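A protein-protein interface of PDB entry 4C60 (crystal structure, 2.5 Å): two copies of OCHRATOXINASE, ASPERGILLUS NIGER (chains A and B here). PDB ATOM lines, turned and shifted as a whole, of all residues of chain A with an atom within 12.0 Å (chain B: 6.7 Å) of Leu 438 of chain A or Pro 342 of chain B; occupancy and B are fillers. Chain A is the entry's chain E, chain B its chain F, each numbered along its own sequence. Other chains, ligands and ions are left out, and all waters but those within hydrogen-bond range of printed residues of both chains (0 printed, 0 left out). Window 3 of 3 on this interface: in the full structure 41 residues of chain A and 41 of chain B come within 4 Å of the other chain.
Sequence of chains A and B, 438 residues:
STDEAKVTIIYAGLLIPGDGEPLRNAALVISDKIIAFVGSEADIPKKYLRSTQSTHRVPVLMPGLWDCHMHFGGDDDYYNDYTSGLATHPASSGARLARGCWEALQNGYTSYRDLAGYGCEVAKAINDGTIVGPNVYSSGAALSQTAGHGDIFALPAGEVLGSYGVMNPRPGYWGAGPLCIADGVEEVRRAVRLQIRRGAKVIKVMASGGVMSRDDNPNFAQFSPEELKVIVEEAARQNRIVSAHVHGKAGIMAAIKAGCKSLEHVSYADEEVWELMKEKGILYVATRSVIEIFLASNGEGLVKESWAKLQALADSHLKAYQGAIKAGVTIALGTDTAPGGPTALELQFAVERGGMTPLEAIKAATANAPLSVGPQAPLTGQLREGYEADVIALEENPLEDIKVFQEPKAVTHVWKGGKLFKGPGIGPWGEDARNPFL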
ATOM      1  N   ASP A 128      -6.382 -19.513  -0.342  1.00  0.00           N
ATOM      2  CA  ASP A 128      -7.772 -19.147  -0.057  1.00  0.00           C
ATOM      3  C   ASP A 128      -8.185 -19.453   1.393  1.00  0.00           C
ATOM      4  O   ASP A 128      -9.322 -19.230   1.769  1.00  0.00           O
ATOM      5  CB  ASP A 128      -8.747 -19.760  -1.080  1.00  0.00           C
ATOM      6  CG  ASP A 128      -8.967 -21.260  -0.901  1.00  0.00           C
ATOM      7  OD1 ASP A 128      -8.429 -21.883   0.046  1.00  0.00           O
ATOM      8  OD2 ASP A 128      -9.727 -21.826  -1.715  1.00  0.00           O
ATOM      9  N   GLY A 129      -7.244 -19.938   2.199  1.00  0.00           N
ATOM     10  CA  GLY A 129      -7.469 -20.167   3.623  1.00  0.00           C
ATOM     11  C   GLY A 129      -8.047 -21.531   3.974  1.00  0.00           C
ATOM     12  O   GLY A 129      -8.181 -21.843   5.154  1.00  0.00           O
ATOM     13  N   THR A 130      -8.399 -22.345   2.975  1.00  0.00           N
ATOM     14  CA  THR A 130      -9.024 -23.653   3.246  1.00  0.00           C
ATOM     15  C   THR A 130      -8.106 -24.586   4.048  1.00  0.00           C
ATOM     16  O   THR A 130      -8.554 -25.213   4.998  1.00  0.00           O
ATOM     17  CB  THR A 130      -9.481 -24.387   1.961  1.00  0.00           C
ATOM     18  OG1 THR A 130     -10.150 -23.480   1.080  1.00  0.00           O
ATOM     19  CG2 THR A 130     -10.442 -25.527   2.306  1.00  0.00           C
ATOM     20  N   ASP A 432      -7.253 -17.404  15.012  1.00  0.00           N
ATOM     21  CA  ASP A 432      -8.526 -16.918  14.457  1.00  0.00           C
ATOM     22  C   ASP A 432      -9.091 -17.795  13.336  1.00  0.00           C
ATOM     23  O   ASP A 432      -9.905 -17.326  12.530  1.00  0.00           O
ATOM     24  CB  ASP A 432      -8.377 -15.474  13.958  1.00  0.00           C
ATOM     25  CG  ASP A 432      -7.832 -14.549  15.026  1.00  0.00           C
ATOM     26  OD1 ASP A 432      -8.366 -14.563  16.166  1.00  0.00           O
ATOM     27  OD2 ASP A 432      -6.869 -13.806  14.741  1.00  0.00           O
ATOM     28  N   ALA A 433      -8.688 -19.063  13.315  1.00  0.00           N
ATOM     29  CA  ALA A 433      -9.145 -19.980  12.308  1.00  0.00           C
ATOM     30  C   ALA A 433     -10.627 -20.162  12.442  1.00  0.00           C
ATOM     31  O   ALA A 433     -11.164 -20.248  13.540  1.00  0.00           O
ATOM     32  CB  ALA A 433      -8.446 -21.324  12.438  1.00  0.00           C
ATOM     33  N   ARG A 434     -11.310 -20.175  11.308  1.00  0.00           N
ATOM     34  CA  ARG A 434     -12.724 -20.507  11.272  1.00  0.00           C
ATOM     35  C   ARG A 434     -12.924 -21.658  10.289  1.00  0.00           C
ATOM     36  O   ARG A 434     -12.115 -21.880   9.401  1.00  0.00           O
ATOM     37  CB  ARG A 434     -13.578 -19.288  10.882  1.00  0.00           C
ATOM     38  CG  ARG A 434     -13.943 -18.321  12.020  1.00  0.00           C
ATOM     39  CD  ARG A 434     -14.428 -16.961  11.530  1.00  0.00           C
ATOM     40  NE  ARG A 434     -15.589 -16.480  12.316  1.00  0.00           N
ATOM     41  CZ  ARG A 434     -16.870 -16.505  11.923  1.00  0.00           C
ATOM     42  NH1 ARG A 434     -17.218 -16.942  10.712  1.00  0.00           N
ATOM     43  NH2 ARG A 434     -17.829 -16.076  12.742  1.00  0.00           N
ATOM     44  N   ASN A 435     -13.994 -22.422  10.484  1.00  0.00           N
ATOM     45  CA  ASN A 435     -14.397 -23.430   9.524  1.00  0.00           C
ATOM     46  C   ASN A 435     -14.746 -22.742   8.199  1.00  0.00           C
ATOM     47  O   ASN A 435     -15.716 -21.988   8.135  1.00  0.00           O
ATOM     48  CB  ASN A 435     -15.604 -24.196  10.071  1.00  0.00           C
ATOM     49  CG  ASN A 435     -16.076 -25.299   9.152  1.00  0.00           C
ATOM     50  OD1 ASN A 435     -15.533 -25.497   8.073  1.00  0.00           O
ATOM     51  ND2 ASN A 435     -17.055 -26.056   9.604  1.00  0.00           N
ATOM     52  N   PRO A 436     -13.951 -22.983   7.142  1.00  0.00           N
ATOM     53  CA  PRO A 436     -14.214 -22.293   5.885  1.00  0.00           C
ATOM     54  C   PRO A 436     -15.514 -22.704   5.203  1.00  0.00           C
ATOM     55  O   PRO A 436     -15.959 -22.008   4.317  1.00  0.00           O
ATOM     56  CB  PRO A 436     -13.027 -22.688   4.990  1.00  0.00           C
ATOM     57  CG  PRO A 436     -12.100 -23.513   5.820  1.00  0.00           C
ATOM     58  CD  PRO A 436     -12.853 -23.958   7.030  1.00  0.00           C
ATOM     59  N   PHE A 437     -16.099 -23.829   5.589  1.00  0.00           N
ATOM     60  CA  PHE A 437     -17.259 -24.366   4.892  1.00  0.00           C
ATOM     61  C   PHE A 437     -18.552 -23.959   5.585  1.00  0.00           C
ATOM     62  O   PHE A 437     -19.638 -24.287   5.096  1.00  0.00           O
ATOM     63  CB  PHE A 437     -17.142 -25.890   4.775  1.00  0.00           C
ATOM     64  CG  PHE A 437     -15.886 -26.332   4.078  1.00  0.00           C
ATOM     65  CD1 PHE A 437     -15.780 -26.257   2.698  1.00  0.00           C
ATOM     66  CD2 PHE A 437     -14.789 -26.761   4.803  1.00  0.00           C
ATOM     67  CE1 PHE A 437     -14.622 -26.628   2.051  1.00  0.00           C
ATOM     68  CE2 PHE A 437     -13.618 -27.132   4.163  1.00  0.00           C
ATOM     69  CZ  PHE A 437     -13.535 -27.064   2.782  1.00  0.00           C
ATOM     70  N   LEU A 438     -18.424 -23.250   6.711  1.00  0.00           N
ATOM     71  CA  LEU A 438     -19.593 -22.742   7.454  1.00  0.00           C
ATOM     72  C   LEU A 438     -19.846 -21.311   6.960  1.00  0.00           C
ATOM     73  O   LEU A 438     -20.931 -20.762   7.242  1.00  0.00           O
ATOM     74  CB  LEU A 438     -19.496 -22.874   9.023  1.00  0.00           C
ATOM     75  CG  LEU A 438     -20.183 -24.122   9.578  1.00  0.00           C
ATOM     76  CD1 LEU A 438     -19.763 -24.390  11.026  1.00  0.00           C
ATOM     77  CD2 LEU A 438     -21.707 -24.030   9.484  1.00  0.00           C
ATOM     78  OXT LEU A 438     -19.001 -20.713   6.204  1.00  0.00           O
ATOM     79  N   ASP B  67     -24.544 -37.824   7.909  1.00  0.00           N
ATOM     80  CA  ASP B  67     -25.261 -37.039   6.912  1.00  0.00           C
ATOM     81  C   ASP B  67     -25.304 -37.848   5.618  1.00  0.00           C
ATOM     82  O   ASP B  67     -24.267 -38.319   5.139  1.00  0.00           O
ATOM     83  CB  ASP B  67     -24.622 -35.672   6.658  1.00  0.00           C
ATOM     84  CG  ASP B  67     -25.575 -34.727   5.951  1.00  0.00           C
ATOM     85  OD1 ASP B  67     -25.716 -34.846   4.715  1.00  0.00           O
ATOM     86  OD2 ASP B  67     -26.215 -33.896   6.642  1.00  0.00           O
ATOM     87  N   GLU B 103     -13.128 -31.268   9.803  1.00  0.00           N
ATOM     88  CA  GLU B 103     -14.128 -30.443  10.450  1.00  0.00           C
ATOM     89  C   GLU B 103     -15.396 -31.245  10.780  1.00  0.00           C
ATOM     90  O   GLU B 103     -16.004 -31.068  11.841  1.00  0.00           O
ATOM     91  CB  GLU B 103     -14.474 -29.261   9.546  1.00  0.00           C
ATOM     92  CG  GLU B 103     -14.642 -27.958  10.267  1.00  0.00           C
ATOM     93  CD  GLU B 103     -13.417 -27.312  10.780  1.00  0.00           C
ATOM     94  OE1 GLU B 103     -12.413 -27.177  10.084  1.00  0.00           O
ATOM     95  OE2 GLU B 103     -13.510 -26.880  11.932  1.00  0.00           O
ATOM     96  N   ASN B 107     -17.061 -32.172  14.536  1.00  0.00           N
ATOM     97  CA  ASN B 107     -18.473 -31.926  14.841  1.00  0.00           C
ATOM     98  C   ASN B 107     -19.278 -33.136  15.248  1.00  0.00           C
ATOM     99  O   ASN B 107     -20.481 -33.018  15.435  1.00  0.00           O
ATOM    100  CB  ASN B 107     -19.179 -31.296  13.635  1.00  0.00           C
ATOM    101  CG  ASN B 107     -19.023 -29.806  13.621  1.00  0.00           C
ATOM    102  OD1 ASN B 107     -19.814 -29.086  14.219  1.00  0.00           O
ATOM    103  ND2 ASN B 107     -17.924 -29.337  13.022  1.00  0.00           N
ATOM    104  N   TYR B 109     -19.579 -36.001  13.300  1.00  0.00           N
ATOM    105  CA  TYR B 109     -20.068 -36.727  12.142  1.00  0.00           C
ATOM    106  C   TYR B 109     -19.083 -37.810  11.753  1.00  0.00           C
ATOM    107  O   TYR B 109     -17.986 -37.509  11.274  1.00  0.00           O
ATOM    108  CB  TYR B 109     -20.332 -35.764  10.991  1.00  0.00           C
ATOM    109  CG  TYR B 109     -21.627 -35.017  11.177  1.00  0.00           C
ATOM    110  CD1 TYR B 109     -21.712 -33.951  12.056  1.00  0.00           C
ATOM    111  CD2 TYR B 109     -22.770 -35.403  10.512  1.00  0.00           C
ATOM    112  CE1 TYR B 109     -22.903 -33.277  12.260  1.00  0.00           C
ATOM    113  CE2 TYR B 109     -23.962 -34.734  10.702  1.00  0.00           C
ATOM    114  CZ  TYR B 109     -24.016 -33.667  11.578  1.00  0.00           C
ATOM    115  OH  TYR B 109     -25.203 -33.016  11.781  1.00  0.00           O
ATOM    116  N   SER B 289     -32.390 -28.167   4.125  1.00  0.00           N
ATOM    117  CA  SER B 289     -31.399 -27.080   4.193  1.00  0.00           C
ATOM    118  C   SER B 289     -31.254 -26.346   2.875  1.00  0.00           C
ATOM    119  O   SER B 289     -31.141 -25.124   2.836  1.00  0.00           O
ATOM    120  CB  SER B 289     -30.021 -27.621   4.603  1.00  0.00           C
ATOM    121  OG  SER B 289     -30.011 -28.035   5.957  1.00  0.00           O
ATOM    122  N   ILE B 293     -31.975 -22.313   2.363  1.00  0.00           N
ATOM    123  CA  ILE B 293     -30.967 -21.382   1.851  1.00  0.00           C
ATOM    124  C   ILE B 293     -31.551 -20.402   0.840  1.00  0.00           C
ATOM    125  O   ILE B 293     -31.377 -19.186   0.985  1.00  0.00           O
ATOM    126  CB  ILE B 293     -29.767 -22.111   1.216  1.00  0.00           C
ATOM    127  CG1 ILE B 293     -28.865 -22.668   2.326  1.00  0.00           C
ATOM    128  CG2 ILE B 293     -28.956 -21.174   0.313  1.00  0.00           C
ATOM    129  CD1 ILE B 293     -27.765 -23.603   1.843  1.00  0.00           C
ATOM    130  N   THR B 335     -28.003 -32.997   4.108  1.00  0.00           N
ATOM    131  CA  THR B 335     -27.960 -31.527   3.990  1.00  0.00           C
ATOM    132  C   THR B 335     -27.794 -31.006   2.538  1.00  0.00           C
ATOM    133  O   THR B 335     -28.333 -29.948   2.194  1.00  0.00           O
ATOM    134  CB  THR B 335     -26.825 -30.962   4.864  1.00  0.00           C
ATOM    135  OG1 THR B 335     -26.926 -31.494   6.191  1.00  0.00           O
ATOM    136  CG2 THR B 335     -26.890 -29.451   4.940  1.00  0.00           C
ATOM    137  N   THR B 337     -24.543 -30.502   1.111  1.00  0.00           N
ATOM    138  CA  THR B 337     -23.473 -29.521   1.273  1.00  0.00           C
ATOM    139  C   THR B 337     -22.080 -30.175   1.153  1.00  0.00           C
ATOM    140  O   THR B 337     -21.952 -31.391   1.011  1.00  0.00           O
ATOM    141  CB  THR B 337     -23.620 -28.810   2.636  1.00  0.00           C
ATOM    142  OG1 THR B 337     -22.788 -27.652   2.696  1.00  0.00           O
ATOM    143  CG2 THR B 337     -23.268 -29.741   3.789  1.00  0.00           C
ATOM    144  N   ALA B 338     -21.047 -29.340   1.141  1.00  0.00           N
ATOM    145  CA  ALA B 338     -19.667 -29.818   1.148  1.00  0.00           C
ATOM    146  C   ALA B 338     -19.322 -30.393   2.535  1.00  0.00           C
ATOM    147  O   ALA B 338     -19.933 -30.002   3.522  1.00  0.00           O
ATOM    148  CB  ALA B 338     -18.716 -28.685   0.799  1.00  0.00           C
ATOM    149  N   GLY B 340     -17.824 -30.755   6.098  1.00  0.00           N
ATOM    150  CA  GLY B 340     -17.614 -29.697   7.079  1.00  0.00           C
ATOM    151  C   GLY B 340     -18.618 -28.561   6.964  1.00  0.00           C
ATOM    152  O   GLY B 340     -18.494 -27.554   7.653  1.00  0.00           O
ATOM    153  N   GLY B 341     -19.622 -28.720   6.103  1.00  0.00           N
ATOM    154  CA  GLY B 341     -20.689 -27.739   5.960  1.00  0.00           C
ATOM    155  C   GLY B 341     -21.645 -27.739   7.143  1.00  0.00           C
ATOM    156  O   GLY B 341     -21.481 -28.504   8.103  1.00  0.00           O
ATOM    157  N   PRO B 342     -22.686 -26.906   7.070  1.00  0.00           N
ATOM    158  CA  PRO B 342     -23.619 -26.741   8.184  1.00  0.00           C
ATOM    159  C   PRO B 342     -24.633 -27.880   8.331  1.00  0.00           C
ATOM    160  O   PRO B 342     -25.841 -27.641   8.314  1.00  0.00           O
ATOM    161  CB  PRO B 342     -24.304 -25.391   7.856  1.00  0.00           C
ATOM    162  CG  PRO B 342     -24.268 -25.289   6.364  1.00  0.00           C
ATOM    163  CD  PRO B 342     -23.003 -26.004   5.939  1.00  0.00           C
ATOM    164  N   THR B 343     -24.146 -29.106   8.457  1.00  0.00           N
ATOM    165  CA  THR B 343     -25.008 -30.292   8.520  1.00  0.00           C
ATOM    166  C   THR B 343     -25.945 -30.334   9.741  1.00  0.00           C
ATOM    167  O   THR B 343     -27.044 -30.883   9.671  1.00  0.00           O
ATOM    168  CB  THR B 343     -24.165 -31.582   8.524  1.00  0.00           C
ATOM    169  OG1 THR B 343     -23.198 -31.515   9.580  1.00  0.00           O
ATOM    170  CG2 THR B 343     -23.454 -31.769   7.204  1.00  0.00           C
ATOM    171  N   ALA B 344     -25.499 -29.765  10.856  1.00  0.00           N
ATOM    172  CA  ALA B 344     -26.276 -29.756  12.100  1.00  0.00           C
ATOM    173  C   ALA B 344     -27.636 -29.050  11.949  1.00  0.00           C
ATOM    174  O   ALA B 344     -28.599 -29.397  12.619  1.00  0.00           O
ATOM    175  CB  ALA B 344     -25.462 -29.103  13.208  1.00  0.00           C
ATOM    176  N   LEU B 345     -27.702 -28.074  11.046  1.00  0.00           N
ATOM    177  CA  LEU B 345     -28.947 -27.355  10.777  1.00  0.00           C
ATOM    178  C   LEU B 345     -30.064 -28.278  10.312  1.00  0.00           C
ATOM    179  O   LEU B 345     -31.238 -28.009  10.547  1.00  0.00           O
ATOM    180  CB  LEU B 345     -28.731 -26.279   9.717  1.00  0.00           C
ATOM    181  CG  LEU B 345     -28.328 -24.900  10.233  1.00  0.00           C
ATOM    182  CD1 LEU B 345     -27.770 -24.027   9.110  1.00  0.00           C
ATOM    183  CD2 LEU B 345     -29.468 -24.179  10.925  1.00  0.00           C
ATOM    184  N   GLU B 346     -29.697 -29.357   9.627  1.00  0.00           N
ATOM    185  CA  GLU B 346     -30.705 -30.287   9.109  1.00  0.00           C
ATOM    186  C   GLU B 346     -31.503 -30.943  10.238  1.00  0.00           C
ATOM    187  O   GLU B 346     -32.700 -31.172  10.094  1.00  0.00           O
ATOM    188  CB  GLU B 346     -30.053 -31.332   8.215  1.00  0.00           C
ATOM    189  CG  GLU B 346     -31.036 -32.171   7.425  1.00  0.00           C
ATOM    190  CD  GLU B 346     -31.799 -31.391   6.381  1.00  0.00           C
ATOM    191  OE1 GLU B 346     -31.332 -30.318   5.936  1.00  0.00           O
ATOM    192  OE2 GLU B 346     -32.884 -31.872   5.992  1.00  0.00           O
ATOM    193  N   PHE B 349     -34.040 -28.388  11.266  1.00  0.00           N
ATOM    194  CA  PHE B 349     -35.158 -28.362  10.322  1.00  0.00           C
ATOM    195  C   PHE B 349     -36.036 -29.598  10.443  1.00  0.00           C
ATOM    196  O   PHE B 349     -37.233 -29.505  10.292  1.00  0.00           O
ATOM    197  CB  PHE B 349     -34.677 -28.185   8.883  1.00  0.00           C
ATOM    198  CG  PHE B 349     -33.941 -26.892   8.641  1.00  0.00           C
ATOM    199  CD1 PHE B 349     -34.417 -25.690   9.166  1.00  0.00           C
ATOM    200  CD2 PHE B 349     -32.760 -26.881   7.882  1.00  0.00           C
ATOM    201  CE1 PHE B 349     -33.731 -24.513   8.960  1.00  0.00           C
ATOM    202  CE2 PHE B 349     -32.075 -25.704   7.665  1.00  0.00           C
ATOM    203  CZ  PHE B 349     -32.560 -24.517   8.204  1.00  0.00           C
ATOM    204  N   GLN B 406     -25.072 -27.380  16.794  1.00  0.00           N
ATOM    205  CA  GLN B 406     -24.510 -26.316  15.961  1.00  0.00           C
ATOM    206  C   GLN B 406     -23.302 -25.641  16.606  1.00  0.00           C
ATOM    207  O   GLN B 406     -22.749 -24.707  16.042  1.00  0.00           O
ATOM    208  CB  GLN B 406     -25.578 -25.285  15.606  1.00  0.00           C
ATOM    209  CG  GLN B 406     -26.675 -25.869  14.735  1.00  0.00           C
ATOM    210  CD  GLN B 406     -27.790 -24.898  14.457  1.00  0.00           C
ATOM    211  OE1 GLN B 406     -27.550 -23.718  14.226  1.00  0.00           O
ATOM    212  NE2 GLN B 406     -29.022 -25.387  14.487  1.00  0.00           N
ATOM    213  N   PRO B 408     -19.743 -26.956  17.686  1.00  0.00           N
ATOM    214  CA  PRO B 408     -18.786 -28.083  17.777  1.00  0.00           C
ATOM    215  C   PRO B 408     -18.031 -28.235  19.115  1.00  0.00           C
ATOM    216  O   PRO B 408     -17.650 -29.348  19.459  1.00  0.00           O
ATOM    217  CB  PRO B 408     -17.790 -27.842  16.629  1.00  0.00           C
ATOM    218  CG  PRO B 408     -18.173 -26.570  15.952  1.00  0.00           C
ATOM    219  CD  PRO B 408     -19.399 -25.991  16.618  1.00  0.00           C
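The backbone carbonyl oxygen of Gly 340 of chain B is in hydrogen-bond range of the side-chain amide nitrogen of Asn 435 of chain A (2.8 Å).
The side-chain amide nitrogen of Asn 107 of chain B is in hydrogen-bond range of the backbone carbonyl oxygen of Glu 103 of chain B, at 2.8 Å.
OD1 of Asn 435 of chain A sits at hydrogen-bond distance from N of Phe 437 of chain A, at 3.0 Å.
Among the printed residues, merely in contact across the chains: Asn 435 of chain A with Glu 103 of chain B (3.1 Å), Phe 437 of chain A with Gly 340 of chain B (3.6 Å), Phe 437 of chain A with Gly 341 of chain B (3.7 Å), Phe 437 of chain A with Pro 342 of chain B (3.9 Å) and Leu 438 of chain A with Pro 342 of chain B (3.4 Å).
Of the printed residues of chain B, Leu 438 of chain A touches Pro 342 (3.4 Å).
Of the printed residues of chain A, Pro 342 of chain B touches Phe 437 (3.9 Å) and Leu 438 (3.4 Å).
No residue of chain A comes within 4 Å of Thr 337 of chain B.
Of chain A, only Phe 437 comes within 4 Å of Gly 341 of chain B.
No residue of chain A comes within 4 Å of Thr 343 of chain B.
No residue of chain A comes within 4 Å of Leu 345 of chain B.
Of the printed residues of chain A, Glu 103 of chain B touches Asn 435 (3.1 Å).
Of the printed residues of chain B, Asn 435 of chain A touches Glu 103 and Gly 340.
Printed residues of chain B within 4 Å of Phe 437 of chain A: Gly 340 (3.6 Å), Gly 341 (3.7 Å) and Pro 342 (3.9 Å).
Pro 408 of chain B touches none of the printed residues of chain A.
The nearest printed residue of chain A that does not touch Glu 103 of chain B is Pro 436 of chain A (4.5 Å).
Hydrophobic or aromatic side chains of chain A that line the printed part of chain B: Phe 437 and Leu 438.
Among the printed residues, 6 pairs touch across the chains.
Among the printed residues, no Asp or Glu carboxylate lies within 4 Å of a Lys or Arg side-chain nitrogen of the other chain.
No position is printed for both chains.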
